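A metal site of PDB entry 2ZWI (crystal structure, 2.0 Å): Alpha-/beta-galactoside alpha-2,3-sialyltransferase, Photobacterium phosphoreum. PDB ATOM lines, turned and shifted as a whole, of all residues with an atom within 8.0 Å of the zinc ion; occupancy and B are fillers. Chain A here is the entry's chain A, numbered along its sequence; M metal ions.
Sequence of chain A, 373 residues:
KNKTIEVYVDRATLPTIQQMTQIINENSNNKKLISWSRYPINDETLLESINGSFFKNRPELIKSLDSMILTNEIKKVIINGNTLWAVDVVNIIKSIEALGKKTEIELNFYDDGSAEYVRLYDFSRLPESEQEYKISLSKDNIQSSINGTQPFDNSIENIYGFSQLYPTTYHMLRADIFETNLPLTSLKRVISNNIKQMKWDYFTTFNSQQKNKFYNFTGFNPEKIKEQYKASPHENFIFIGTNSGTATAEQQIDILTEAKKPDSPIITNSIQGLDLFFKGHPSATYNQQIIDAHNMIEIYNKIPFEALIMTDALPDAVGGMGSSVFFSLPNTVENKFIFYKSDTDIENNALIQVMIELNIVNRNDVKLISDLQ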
ATOM      1  N   TYR A 229     -24.242  13.650 -25.158  1.00  0.00           N
ATOM      2  CA  TYR A 229     -25.284  12.686 -24.838  1.00  0.00           C
ATOM      3  C   TYR A 229     -25.755  11.891 -26.070  1.00  0.00           C
ATOM      4  O   TYR A 229     -25.958  10.679 -25.988  1.00  0.00           O
ATOM      5  CB  TYR A 229     -26.493  13.399 -24.219  1.00  0.00           C
ATOM      6  CG  TYR A 229     -26.341  13.837 -22.767  1.00  0.00           C
ATOM      7  CD1 TYR A 229     -25.478  13.171 -21.898  1.00  0.00           C
ATOM      8  CD2 TYR A 229     -27.122  14.886 -22.256  1.00  0.00           C
ATOM      9  CE1 TYR A 229     -25.353  13.582 -20.553  1.00  0.00           C
ATOM     10  CE2 TYR A 229     -26.996  15.296 -20.912  1.00  0.00           C
ATOM     11  CZ  TYR A 229     -26.123  14.643 -20.083  1.00  0.00           C
ATOM     12  OH  TYR A 229     -26.003  15.036 -18.755  1.00  0.00           O
ATOM     13  N   ALA A 231     -24.207  11.576 -29.131  1.00  0.00           N
ATOM     14  CA  ALA A 231     -23.139  11.150 -30.033  1.00  0.00           C
ATOM     15  C   ALA A 231     -23.149   9.648 -30.303  1.00  0.00           C
ATOM     16  O   ALA A 231     -22.846   9.201 -31.410  1.00  0.00           O
ATOM     17  CB  ALA A 231     -21.780  11.593 -29.491  1.00  0.00           C
ATOM     18  N   SER A 232     -23.513   8.874 -29.282  1.00  0.00           N
ATOM     19  CA  SER A 232     -23.645   7.428 -29.389  1.00  0.00           C
ATOM     20  C   SER A 232     -25.050   7.052 -28.920  1.00  0.00           C
ATOM     21  O   SER A 232     -25.647   7.773 -28.108  1.00  0.00           O
ATOM     22  CB  SER A 232     -22.533   6.738 -28.594  1.00  0.00           C
ATOM     23  OG  SER A 232     -22.986   5.621 -27.845  1.00  0.00           O
ATOM     24  N   PRO A 233     -25.622   5.959 -29.460  1.00  0.00           N
ATOM     25  CA  PRO A 233     -27.015   5.664 -29.133  1.00  0.00           C
ATOM     26  C   PRO A 233     -27.203   4.996 -27.772  1.00  0.00           C
ATOM     27  O   PRO A 233     -28.331   4.718 -27.362  1.00  0.00           O
ATOM     28  CB  PRO A 233     -27.419   4.695 -30.244  1.00  0.00           C
ATOM     29  CG  PRO A 233     -26.145   3.950 -30.553  1.00  0.00           C
ATOM     30  CD  PRO A 233     -25.044   4.952 -30.385  1.00  0.00           C
ATOM     31  N   HIS A 234     -26.101   4.725 -27.069  1.00  0.00           N
ATOM     32  CA  HIS A 234     -26.177   4.046 -25.776  1.00  0.00           C
ATOM     33  C   HIS A 234     -26.659   5.010 -24.696  1.00  0.00           C
ATOM     34  O   HIS A 234     -26.479   6.220 -24.800  1.00  0.00           O
ATOM     35  CB  HIS A 234     -24.831   3.423 -25.428  1.00  0.00           C
ATOM     36  CG  HIS A 234     -24.300   2.526 -26.501  1.00  0.00           C
ATOM     37  ND1 HIS A 234     -23.049   2.693 -27.065  1.00  0.00           N
ATOM     38  CD2 HIS A 234     -24.860   1.473 -27.147  1.00  0.00           C
ATOM     39  CE1 HIS A 234     -22.865   1.771 -27.992  1.00  0.00           C
ATOM     40  NE2 HIS A 234     -23.944   1.022 -28.065  1.00  0.00           N
ATOM     41  N   GLU A 235     -27.292   4.461 -23.654  1.00  0.00           N
ATOM     42  CA  GLU A 235     -27.789   5.292 -22.551  1.00  0.00           C
ATOM     43  C   GLU A 235     -26.617   5.922 -21.779  1.00  0.00           C
ATOM     44  O   GLU A 235     -25.518   5.375 -21.749  1.00  0.00           O
ATOM     45  CB  GLU A 235     -28.731   4.514 -21.636  1.00  0.00           C
ATOM     46  CG  GLU A 235     -30.034   4.117 -22.367  1.00  0.00           C
ATOM     47  CD  GLU A 235     -31.176   3.832 -21.423  1.00  0.00           C
ATOM     48  OE1 GLU A 235     -30.969   3.096 -20.431  1.00  0.00           O
ATOM     49  OE2 GLU A 235     -32.296   4.351 -21.684  1.00  0.00           O
ATOM     50  N   ASN A 236     -26.883   7.071 -21.174  1.00  0.00           N
ATOM     51  CA  ASN A 236     -25.856   7.924 -20.601  1.00  0.00           C
ATOM     52  C   ASN A 236     -25.797   7.805 -19.082  1.00  0.00           C
ATOM     53  O   ASN A 236     -26.826   7.884 -18.416  1.00  0.00           O
ATOM     54  CB  ASN A 236     -26.129   9.380 -21.003  1.00  0.00           C
ATOM     55  CG  ASN A 236     -26.129   9.575 -22.515  1.00  0.00           C
ATOM     56  OD1 ASN A 236     -25.179   9.207 -23.194  1.00  0.00           O
ATOM     57  ND2 ASN A 236     -27.184  10.185 -23.038  1.00  0.00           N
ATOM     58  N   GLY A 273     -21.628  -1.210 -20.654  1.00  0.00           N
ATOM     59  CA  GLY A 273     -22.292  -0.853 -21.911  1.00  0.00           C
ATOM     60  C   GLY A 273     -22.942   0.530 -21.965  1.00  0.00           C
ATOM     61  O   GLY A 273     -23.563   0.881 -22.974  1.00  0.00           O
ATOM     62  N   LEU A 274     -22.825   1.322 -20.901  1.00  0.00           N
ATOM     63  CA  LEU A 274     -23.323   2.689 -20.902  1.00  0.00           C
ATOM     64  C   LEU A 274     -22.253   3.674 -21.385  1.00  0.00           C
ATOM     65  O   LEU A 274     -21.061   3.391 -21.283  1.00  0.00           O
ATOM     66  CB  LEU A 274     -23.849   3.092 -19.520  1.00  0.00           C
ATOM     67  CG  LEU A 274     -24.974   2.255 -18.900  1.00  0.00           C
ATOM     68  CD1 LEU A 274     -25.469   2.877 -17.622  1.00  0.00           C
ATOM     69  CD2 LEU A 274     -26.142   2.044 -19.882  1.00  0.00           C
ATOM     70  N   ASP A 275     -22.677   4.818 -21.931  1.00  0.00           N
ATOM     71  CA  ASP A 275     -21.738   5.909 -22.199  1.00  0.00           C
ATOM     72  C   ASP A 275     -21.445   6.604 -20.861  1.00  0.00           C
ATOM     73  O   ASP A 275     -22.368   7.112 -20.205  1.00  0.00           O
ATOM     74  CB  ASP A 275     -22.321   6.894 -23.220  1.00  0.00           C
ATOM     75  CG  ASP A 275     -22.516   6.257 -24.586  1.00  0.00           C
ATOM     76  OD1 ASP A 275     -21.932   5.189 -24.824  1.00  0.00           O
ATOM     77  OD2 ASP A 275     -23.258   6.816 -25.425  1.00  0.00           O
ATOM     78  N   LEU A 276     -20.180   6.572 -20.452  1.00  0.00           N
ATOM     79  CA  LEU A 276     -19.799   7.020 -19.116  1.00  0.00           C
ATOM     80  C   LEU A 276     -19.268   8.450 -19.132  1.00  0.00           C
ATOM     81  O   LEU A 276     -18.377   8.768 -19.909  1.00  0.00           O
ATOM     82  CB  LEU A 276     -18.741   6.094 -18.529  1.00  0.00           C
ATOM     83  CG  LEU A 276     -19.018   4.598 -18.472  1.00  0.00           C
ATOM     84  CD1 LEU A 276     -17.864   3.935 -17.687  1.00  0.00           C
ATOM     85  CD2 LEU A 276     -20.392   4.289 -17.829  1.00  0.00           C
ATOM     86  N   ILE A 297     -16.041  10.517 -20.506  1.00  0.00           N
ATOM     87  CA  ILE A 297     -16.300  11.847 -21.052  1.00  0.00           C
ATOM     88  C   ILE A 297     -16.344  12.861 -19.892  1.00  0.00           C
ATOM     89  O   ILE A 297     -17.187  12.757 -19.010  1.00  0.00           O
ATOM     90  CB  ILE A 297     -17.615  11.897 -21.868  1.00  0.00           C
ATOM     91  CG1 ILE A 297     -17.590  10.858 -22.995  1.00  0.00           C
ATOM     92  CG2 ILE A 297     -17.867  13.294 -22.413  1.00  0.00           C
ATOM     93  CD1 ILE A 297     -18.816  10.895 -23.877  1.00  0.00           C
HETATM   94 ZN    ZN M   1     -21.675   4.128 -26.545  1.00  0.00          ZN
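The zinc ion is bound by OD1 of Asp 275 (2.0 Å), ND1 of His 234 (2.1 Å) and OG of Ser 232 (2.4 Å). The zinc ion has three donor atoms within binding distance.
O of Glu 235 is in hydrogen-bond range of N of Asp 275, at 2.9 Å.
Within 4 Å of the zinc ion: Ser 232, His 234 and Asp 275.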
